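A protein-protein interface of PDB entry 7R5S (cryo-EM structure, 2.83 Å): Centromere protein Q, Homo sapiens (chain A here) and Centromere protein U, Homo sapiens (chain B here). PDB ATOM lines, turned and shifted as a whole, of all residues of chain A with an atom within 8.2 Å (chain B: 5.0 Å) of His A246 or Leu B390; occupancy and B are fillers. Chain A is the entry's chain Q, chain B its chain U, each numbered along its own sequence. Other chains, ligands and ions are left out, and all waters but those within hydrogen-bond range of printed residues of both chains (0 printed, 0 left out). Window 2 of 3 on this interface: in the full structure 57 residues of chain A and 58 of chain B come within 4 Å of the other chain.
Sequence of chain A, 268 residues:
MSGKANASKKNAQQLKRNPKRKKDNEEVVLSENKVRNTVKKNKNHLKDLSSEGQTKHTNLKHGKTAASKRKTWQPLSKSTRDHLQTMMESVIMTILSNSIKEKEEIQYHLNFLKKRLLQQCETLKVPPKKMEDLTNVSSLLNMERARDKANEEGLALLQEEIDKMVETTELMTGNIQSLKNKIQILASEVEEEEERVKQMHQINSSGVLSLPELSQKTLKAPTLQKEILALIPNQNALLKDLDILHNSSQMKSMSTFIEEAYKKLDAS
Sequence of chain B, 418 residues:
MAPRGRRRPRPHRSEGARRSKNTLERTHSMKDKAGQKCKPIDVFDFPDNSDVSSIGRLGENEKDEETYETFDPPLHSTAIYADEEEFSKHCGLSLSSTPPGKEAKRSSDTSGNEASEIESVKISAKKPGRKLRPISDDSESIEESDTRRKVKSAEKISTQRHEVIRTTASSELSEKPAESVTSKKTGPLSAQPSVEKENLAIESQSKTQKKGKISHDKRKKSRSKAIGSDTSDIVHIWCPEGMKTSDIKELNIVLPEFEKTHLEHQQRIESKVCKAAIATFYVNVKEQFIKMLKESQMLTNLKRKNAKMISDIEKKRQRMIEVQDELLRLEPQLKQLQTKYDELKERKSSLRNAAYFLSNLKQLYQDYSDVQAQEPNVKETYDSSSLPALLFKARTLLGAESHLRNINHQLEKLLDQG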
ATOM      1  N   ILE A 228      26.751 -34.023 -21.546  1.00  0.00           N
ATOM      2  CA  ILE A 228      27.212 -32.832 -22.254  1.00  0.00           C
ATOM      3  C   ILE A 228      27.933 -31.890 -21.297  1.00  0.00           C
ATOM      4  O   ILE A 228      29.007 -31.366 -21.611  1.00  0.00           O
ATOM      5  CB  ILE A 228      26.033 -32.130 -22.953  1.00  0.00           C
ATOM      6  CG1 ILE A 228      25.564 -32.945 -24.159  1.00  0.00           C
ATOM      7  CG2 ILE A 228      26.427 -30.725 -23.384  1.00  0.00           C
ATOM      8  CD1 ILE A 228      24.461 -32.275 -24.953  1.00  0.00           C
ATOM      9  N   GLN A 235      32.637 -23.709 -20.379  1.00  0.00           N
ATOM     10  CA  GLN A 235      31.232 -23.443 -20.674  1.00  0.00           C
ATOM     11  C   GLN A 235      30.992 -22.001 -21.111  1.00  0.00           C
ATOM     12  O   GLN A 235      30.585 -21.749 -22.251  1.00  0.00           O
ATOM     13  CB  GLN A 235      30.367 -23.759 -19.451  1.00  0.00           C
ATOM     14  CG  GLN A 235      30.001 -25.226 -19.299  1.00  0.00           C
ATOM     15  CD  GLN A 235      31.204 -26.096 -18.999  1.00  0.00           C
ATOM     16  OE1 GLN A 235      31.827 -26.647 -19.905  1.00  0.00           O
ATOM     17  NE2 GLN A 235      31.540 -26.221 -17.721  1.00  0.00           N
ATOM     18  N   LEU A 238      32.846 -20.709 -24.039  1.00  0.00           N
ATOM     19  CA  LEU A 238      32.267 -21.051 -25.331  1.00  0.00           C
ATOM     20  C   LEU A 238      30.975 -20.282 -25.582  1.00  0.00           C
ATOM     21  O   LEU A 238      30.645 -19.992 -26.737  1.00  0.00           O
ATOM     22  CB  LEU A 238      32.041 -22.565 -25.418  1.00  0.00           C
ATOM     23  CG  LEU A 238      31.503 -23.193 -26.710  1.00  0.00           C
ATOM     24  CD1 LEU A 238      31.981 -24.625 -26.809  1.00  0.00           C
ATOM     25  CD2 LEU A 238      29.981 -23.172 -26.778  1.00  0.00           C
ATOM     26  N   LEU A 239      30.246 -19.936 -24.518  1.00  0.00           N
ATOM     27  CA  LEU A 239      28.999 -19.194 -24.679  1.00  0.00           C
ATOM     28  C   LEU A 239      29.251 -17.745 -25.088  1.00  0.00           C
ATOM     29  O   LEU A 239      28.387 -17.128 -25.724  1.00  0.00           O
ATOM     30  CB  LEU A 239      28.193 -19.253 -23.378  1.00  0.00           C
ATOM     31  CG  LEU A 239      27.015 -18.298 -23.148  1.00  0.00           C
ATOM     32  CD1 LEU A 239      25.943 -18.452 -24.226  1.00  0.00           C
ATOM     33  CD2 LEU A 239      26.423 -18.486 -21.757  1.00  0.00           C
ATOM     34  N   LYS A 240      30.429 -17.204 -24.754  1.00  0.00           N
ATOM     35  CA  LYS A 240      30.716 -15.783 -24.953  1.00  0.00           C
ATOM     36  C   LYS A 240      30.426 -15.306 -26.375  1.00  0.00           C
ATOM     37  O   LYS A 240      30.028 -14.155 -26.582  1.00  0.00           O
ATOM     38  CB  LYS A 240      32.171 -15.476 -24.574  1.00  0.00           C
ATOM     39  CG  LYS A 240      33.217 -15.893 -25.603  1.00  0.00           C
ATOM     40  CD  LYS A 240      34.558 -16.194 -24.952  1.00  0.00           C
ATOM     41  CE  LYS A 240      35.603 -16.584 -25.989  1.00  0.00           C
ATOM     42  NZ  LYS A 240      35.187 -17.781 -26.772  1.00  0.00           N
ATOM     43  N   ASP A 241      30.638 -16.165 -27.372  1.00  0.00           N
ATOM     44  CA  ASP A 241      30.243 -15.846 -28.736  1.00  0.00           C
ATOM     45  C   ASP A 241      29.155 -16.770 -29.259  1.00  0.00           C
ATOM     46  O   ASP A 241      28.592 -16.499 -30.326  1.00  0.00           O
ATOM     47  CB  ASP A 241      31.452 -15.897 -29.681  1.00  0.00           C
ATOM     48  CG  ASP A 241      31.147 -15.307 -31.046  1.00  0.00           C
ATOM     49  OD1 ASP A 241      31.017 -14.068 -31.139  1.00  0.00           O
ATOM     50  OD2 ASP A 241      31.006 -16.076 -32.018  1.00  0.00           O
ATOM     51  N   LEU A 242      28.852 -17.856 -28.545  1.00  0.00           N
ATOM     52  CA  LEU A 242      27.697 -18.665 -28.907  1.00  0.00           C
ATOM     53  C   LEU A 242      26.415 -17.849 -28.812  1.00  0.00           C
ATOM     54  O   LEU A 242      25.552 -17.944 -29.692  1.00  0.00           O
ATOM     55  CB  LEU A 242      27.630 -19.906 -28.015  1.00  0.00           C
ATOM     56  CG  LEU A 242      26.296 -20.638 -27.857  1.00  0.00           C
ATOM     57  CD1 LEU A 242      25.815 -21.195 -29.183  1.00  0.00           C
ATOM     58  CD2 LEU A 242      26.447 -21.755 -26.847  1.00  0.00           C
ATOM     59  N   ASP A 243      26.297 -17.009 -27.782  1.00  0.00           N
ATOM     60  CA  ASP A 243      25.142 -16.122 -27.689  1.00  0.00           C
ATOM     61  C   ASP A 243      25.122 -15.127 -28.844  1.00  0.00           C
ATOM     62  O   ASP A 243      24.060 -14.839 -29.408  1.00  0.00           O
ATOM     63  CB  ASP A 243      25.145 -15.385 -26.350  1.00  0.00           C
ATOM     64  CG  ASP A 243      26.498 -14.798 -26.011  1.00  0.00           C
ATOM     65  OD1 ASP A 243      26.673 -14.322 -24.870  1.00  0.00           O
ATOM     66  OD2 ASP A 243      27.384 -14.802 -26.891  1.00  0.00           O
ATOM     67  N   ILE A 244      26.292 -14.604 -29.219  1.00  0.00           N
ATOM     68  CA  ILE A 244      26.363 -13.631 -30.305  1.00  0.00           C
ATOM     69  C   ILE A 244      25.914 -14.259 -31.619  1.00  0.00           C
ATOM     70  O   ILE A 244      25.115 -13.678 -32.363  1.00  0.00           O
ATOM     71  CB  ILE A 244      27.786 -13.055 -30.409  1.00  0.00           C
ATOM     72  CG1 ILE A 244      28.083 -12.148 -29.213  1.00  0.00           C
ATOM     73  CG2 ILE A 244      27.964 -12.297 -31.717  1.00  0.00           C
ATOM     74  CD1 ILE A 244      29.443 -11.489 -29.267  1.00  0.00           C
ATOM     75  N   LEU A 245      26.420 -15.456 -31.925  1.00  0.00           N
ATOM     76  CA  LEU A 245      26.014 -16.139 -33.149  1.00  0.00           C
ATOM     77  C   LEU A 245      24.558 -16.590 -33.091  1.00  0.00           C
ATOM     78  O   LEU A 245      23.926 -16.760 -34.139  1.00  0.00           O
ATOM     79  CB  LEU A 245      26.961 -17.310 -33.431  1.00  0.00           C
ATOM     80  CG  LEU A 245      27.051 -18.502 -32.474  1.00  0.00           C
ATOM     81  CD1 LEU A 245      25.996 -19.560 -32.750  1.00  0.00           C
ATOM     82  CD2 LEU A 245      28.446 -19.110 -32.529  1.00  0.00           C
ATOM     83  N   HIS A 246      24.010 -16.792 -31.888  1.00  0.00           N
ATOM     84  CA  HIS A 246      22.565 -16.976 -31.773  1.00  0.00           C
ATOM     85  C   HIS A 246      21.810 -15.668 -31.970  1.00  0.00           C
ATOM     86  O   HIS A 246      20.599 -15.687 -32.216  1.00  0.00           O
ATOM     87  CB  HIS A 246      22.207 -17.598 -30.425  1.00  0.00           C
ATOM     88  CG  HIS A 246      22.131 -19.092 -30.455  1.00  0.00           C
ATOM     89  ND1 HIS A 246      23.160 -19.883 -30.919  1.00  0.00           N
ATOM     90  CD2 HIS A 246      21.137 -19.939 -30.097  1.00  0.00           C
ATOM     91  CE1 HIS A 246      22.807 -21.153 -30.835  1.00  0.00           C
ATOM     92  NE2 HIS A 246      21.585 -21.214 -30.339  1.00  0.00           N
ATOM     93  N   ASN A 247      22.487 -14.528 -31.830  1.00  0.00           N
ATOM     94  CA  ASN A 247      21.859 -13.250 -32.142  1.00  0.00           C
ATOM     95  C   ASN A 247      22.147 -12.781 -33.562  1.00  0.00           C
ATOM     96  O   ASN A 247      21.452 -11.884 -34.054  1.00  0.00           O
ATOM     97  CB  ASN A 247      22.303 -12.179 -31.145  1.00  0.00           C
ATOM     98  CG  ASN A 247      22.156 -12.625 -29.705  1.00  0.00           C
ATOM     99  OD1 ASN A 247      21.354 -13.506 -29.395  1.00  0.00           O
ATOM    100  ND2 ASN A 247      22.933 -12.022 -28.814  1.00  0.00           N
ATOM    101  N   SER A 248      23.141 -13.362 -34.230  1.00  0.00           N
ATOM    102  CA  SER A 248      23.475 -12.949 -35.587  1.00  0.00           C
ATOM    103  C   SER A 248      22.383 -13.387 -36.556  1.00  0.00           C
ATOM    104  O   SER A 248      21.937 -14.537 -36.526  1.00  0.00           O
ATOM    105  CB  SER A 248      24.825 -13.533 -36.003  1.00  0.00           C
ATOM    106  OG  SER A 248      25.787 -13.383 -34.972  1.00  0.00           O
ATOM    107  N   SER A 249      21.952 -12.461 -37.414  1.00  0.00           N
ATOM    108  CA  SER A 249      20.882 -12.727 -38.369  1.00  0.00           C
ATOM    109  C   SER A 249      21.356 -13.476 -39.607  1.00  0.00           C
ATOM    110  O   SER A 249      20.517 -13.968 -40.371  1.00  0.00           O
ATOM    111  CB  SER A 249      20.217 -11.414 -38.791  1.00  0.00           C
ATOM    112  OG  SER A 249      21.092 -10.632 -39.584  1.00  0.00           O
ATOM    113  N   GLN A 250      22.669 -13.572 -39.826  1.00  0.00           N
ATOM    114  CA  GLN A 250      23.180 -14.331 -40.962  1.00  0.00           C
ATOM    115  C   GLN A 250      22.792 -15.800 -40.851  1.00  0.00           C
ATOM    116  O   GLN A 250      22.214 -16.377 -41.782  1.00  0.00           O
ATOM    117  CB  GLN A 250      24.699 -14.180 -41.051  1.00  0.00           C
ATOM    118  CG  GLN A 250      25.183 -12.757 -41.264  1.00  0.00           C
ATOM    119  CD  GLN A 250      25.342 -11.992 -39.966  1.00  0.00           C
ATOM    120  OE1 GLN A 250      24.676 -12.287 -38.974  1.00  0.00           O
ATOM    121  NE2 GLN A 250      26.224 -11.001 -39.967  1.00  0.00           N
ATOM    122  N   MET A 251      23.092 -16.421 -39.707  1.00  0.00           N
ATOM    123  CA  MET A 251      22.671 -17.795 -39.486  1.00  0.00           C
ATOM    124  C   MET A 251      21.156 -17.930 -39.443  1.00  0.00           C
ATOM    125  O   MET A 251      20.631 -18.975 -39.832  1.00  0.00           O
ATOM    126  CB  MET A 251      23.277 -18.339 -38.190  1.00  0.00           C
ATOM    127  CG  MET A 251      22.828 -19.753 -37.864  1.00  0.00           C
ATOM    128  SD  MET A 251      22.907 -20.865 -39.285  1.00  0.00           S
ATOM    129  CE  MET A 251      21.684 -22.088 -38.819  1.00  0.00           C
ATOM    130  N   LYS A 252      20.437 -16.897 -39.007  1.00  0.00           N
ATOM    131  CA  LYS A 252      18.980 -16.978 -39.010  1.00  0.00           C
ATOM    132  C   LYS A 252      18.444 -17.063 -40.433  1.00  0.00           C
ATOM    133  O   LYS A 252      17.579 -17.892 -40.732  1.00  0.00           O
ATOM    134  CB  LYS A 252      18.378 -15.786 -38.265  1.00  0.00           C
ATOM    135  CG  LYS A 252      18.878 -15.621 -36.833  1.00  0.00           C
ATOM    136  CD  LYS A 252      19.147 -16.973 -36.181  1.00  0.00           C
ATOM    137  CE  LYS A 252      20.100 -16.856 -35.013  1.00  0.00           C
ATOM    138  NZ  LYS A 252      20.236 -18.153 -34.293  1.00  0.00           N
ATOM    139  N   SER B 386      21.742 -24.164 -20.011  1.00  0.00           N
ATOM    140  CA  SER B 386      21.155 -23.943 -21.326  1.00  0.00           C
ATOM    141  C   SER B 386      22.113 -24.246 -22.472  1.00  0.00           C
ATOM    142  O   SER B 386      21.697 -24.210 -23.634  1.00  0.00           O
ATOM    143  CB  SER B 386      20.658 -22.498 -21.443  1.00  0.00           C
ATOM    144  OG  SER B 386      19.675 -22.220 -20.461  1.00  0.00           O
ATOM    145  N   LEU B 387      23.373 -24.552 -22.177  1.00  0.00           N
ATOM    146  CA  LEU B 387      24.362 -24.838 -23.211  1.00  0.00           C
ATOM    147  C   LEU B 387      24.087 -26.125 -23.987  1.00  0.00           C
ATOM    148  O   LEU B 387      24.410 -26.185 -25.178  1.00  0.00           O
ATOM    149  CB  LEU B 387      25.772 -24.886 -22.620  1.00  0.00           C
ATOM    150  CG  LEU B 387      26.461 -23.545 -22.347  1.00  0.00           C
ATOM    151  CD1 LEU B 387      25.806 -22.738 -21.234  1.00  0.00           C
ATOM    152  CD2 LEU B 387      27.930 -23.772 -22.062  1.00  0.00           C
ATOM    153  N   PRO B 388      23.545 -27.186 -23.373  1.00  0.00           N
ATOM    154  CA  PRO B 388      23.148 -28.343 -24.195  1.00  0.00           C
ATOM    155  C   PRO B 388      22.132 -27.998 -25.271  1.00  0.00           C
ATOM    156  O   PRO B 388      22.297 -28.407 -26.429  1.00  0.00           O
ATOM    157  CB  PRO B 388      22.579 -29.322 -23.160  1.00  0.00           C
ATOM    158  CG  PRO B 388      23.324 -29.009 -21.927  1.00  0.00           C
ATOM    159  CD  PRO B 388      23.518 -27.520 -21.935  1.00  0.00           C
ATOM    160  N   ALA B 389      21.083 -27.247 -24.927  1.00  0.00           N
ATOM    161  CA  ALA B 389      20.092 -26.871 -25.930  1.00  0.00           C
ATOM    162  C   ALA B 389      20.681 -25.906 -26.952  1.00  0.00           C
ATOM    163  O   ALA B 389      20.331 -25.954 -28.136  1.00  0.00           O
ATOM    164  CB  ALA B 389      18.864 -26.261 -25.257  1.00  0.00           C
ATOM    165  N   LEU B 390      21.590 -25.031 -26.515  1.00  0.00           N
ATOM    166  CA  LEU B 390      22.262 -24.135 -27.451  1.00  0.00           C
ATOM    167  C   LEU B 390      23.113 -24.919 -28.442  1.00  0.00           C
ATOM    168  O   LEU B 390      23.148 -24.599 -29.637  1.00  0.00           O
ATOM    169  CB  LEU B 390      23.119 -23.130 -26.682  1.00  0.00           C
ATOM    170  CG  LEU B 390      22.378 -22.019 -25.932  1.00  0.00           C
ATOM    171  CD1 LEU B 390      23.337 -21.225 -25.058  1.00  0.00           C
ATOM    172  CD2 LEU B 390      21.647 -21.101 -26.896  1.00  0.00           C
ATOM    173  N   LEU B 391      23.797 -25.962 -27.967  1.00  0.00           N
ATOM    174  CA  LEU B 391      24.599 -26.792 -28.855  1.00  0.00           C
ATOM    175  C   LEU B 391      23.718 -27.601 -29.798  1.00  0.00           C
ATOM    176  O   LEU B 391      24.064 -27.793 -30.967  1.00  0.00           O
ATOM    177  CB  LEU B 391      25.504 -27.716 -28.041  1.00  0.00           C
ATOM    178  CG  LEU B 391      26.958 -27.265 -27.881  1.00  0.00           C
ATOM    179  CD1 LEU B 391      27.769 -28.311 -27.133  1.00  0.00           C
ATOM    180  CD2 LEU B 391      27.580 -26.967 -29.238  1.00  0.00           C
ATOM    181  N   PHE B 392      22.569 -28.075 -29.317  1.00  0.00           N
ATOM    182  CA  PHE B 392      21.659 -28.780 -30.211  1.00  0.00           C
ATOM    183  C   PHE B 392      20.990 -27.842 -31.209  1.00  0.00           C
ATOM    184  O   PHE B 392      20.529 -28.302 -32.260  1.00  0.00           O
ATOM    185  CB  PHE B 392      20.602 -29.542 -29.414  1.00  0.00           C
ATOM    186  CG  PHE B 392      20.765 -31.032 -29.478  1.00  0.00           C
ATOM    187  CD1 PHE B 392      21.871 -31.645 -28.915  1.00  0.00           C
ATOM    188  CD2 PHE B 392      19.829 -31.818 -30.130  1.00  0.00           C
ATOM    189  CE1 PHE B 392      22.030 -33.015 -28.979  1.00  0.00           C
ATOM    190  CE2 PHE B 392      19.985 -33.189 -30.201  1.00  0.00           C
ATOM    191  CZ  PHE B 392      21.087 -33.788 -29.623  1.00  0.00           C
ATOM    192  N   LYS B 393      20.920 -26.546 -30.903  1.00  0.00           N
ATOM    193  CA  LYS B 393      20.451 -25.576 -31.886  1.00  0.00           C
ATOM    194  C   LYS B 393      21.538 -25.252 -32.906  1.00  0.00           C
ATOM    195  O   LYS B 393      21.244 -25.049 -34.089  1.00  0.00           O
ATOM    196  CB  LYS B 393      19.980 -24.301 -31.187  1.00  0.00           C
ATOM    197  CG  LYS B 393      18.555 -24.368 -30.663  1.00  0.00           C
ATOM    198  CD  LYS B 393      18.071 -23.000 -30.213  1.00  0.00           C
ATOM    199  CE  LYS B 393      16.580 -23.008 -29.917  1.00  0.00           C
ATOM    200  NZ  LYS B 393      16.089 -21.655 -29.533  1.00  0.00           N
ATOM    201  N   ALA B 394      22.796 -25.191 -32.462  1.00  0.00           N
ATOM    202  CA  ALA B 394      23.920 -25.010 -33.374  1.00  0.00           C
ATOM    203  C   ALA B 394      24.274 -26.286 -34.128  1.00  0.00           C
ATOM    204  O   ALA B 394      25.150 -26.250 -35.000  1.00  0.00           O
ATOM    205  CB  ALA B 394      25.145 -24.507 -32.608  1.00  0.00           C
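O of Leu A242 sits at hydrogen-bond distance from ND1 of His A246 (3.3 Å). O of His A246 lies close to NZ of Lys A252, 3.2 Å away.
Ile A228 touches Pro B388. O of Gln A235 touches CD2 of Leu B387, at 3.3 Å. CD1 of Leu A239 touches CD1 of Leu B390, at 3.9 Å. Leu B390 touches Leu A242 (CB to CD2, 3.6 Å). His A246 touches Leu B390. CB of Lys B393 touches NE2 of His A246, at 3.6 Å.
Leu B390 touches just these residues of chain A: Leu A239 (3.9 Å), Leu A242 (3.6 Å) and His A246 (3.4 Å). No residue of chain A comes within 4 Å of Ala B389. Printed residues of chain B within 4 Å of Gln A235: Leu B387. Printed residues of chain B within 4 Å of Ile A228: Pro B388 (3.8 Å). Of the printed residues of chain A, Lys B393 touches His A246. Of the printed residues of chain A, Leu B387 touches Gln A235. Of the printed residues of chain B, Leu A239 touches Leu B390. Leu B391 touches none of the printed residues of chain A. Asn A247 touches none of the printed residues of chain B. The nearest residue of chain B that does not touch His A246 is Ala B394 (4.4 Å). The nearest printed residue of chain B that does not touch Ile A228 is Leu B391 (4.7 Å).
Of the 9 printed residues of chain B, 4 touch a printed residue of chain A. Hydrophobic or aromatic side chains of chain B within 4 Å of the printed part of chain A: Leu B387, Pro B388 and Leu B390. Hydrophobic or aromatic side chains of chain A within 4 Å of the printed part of chain B: Ile A228, Leu A239, Leu A242 and His A246. Along chain A the printed residues that touch a printed residue of chain B span positions 228 to 246.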
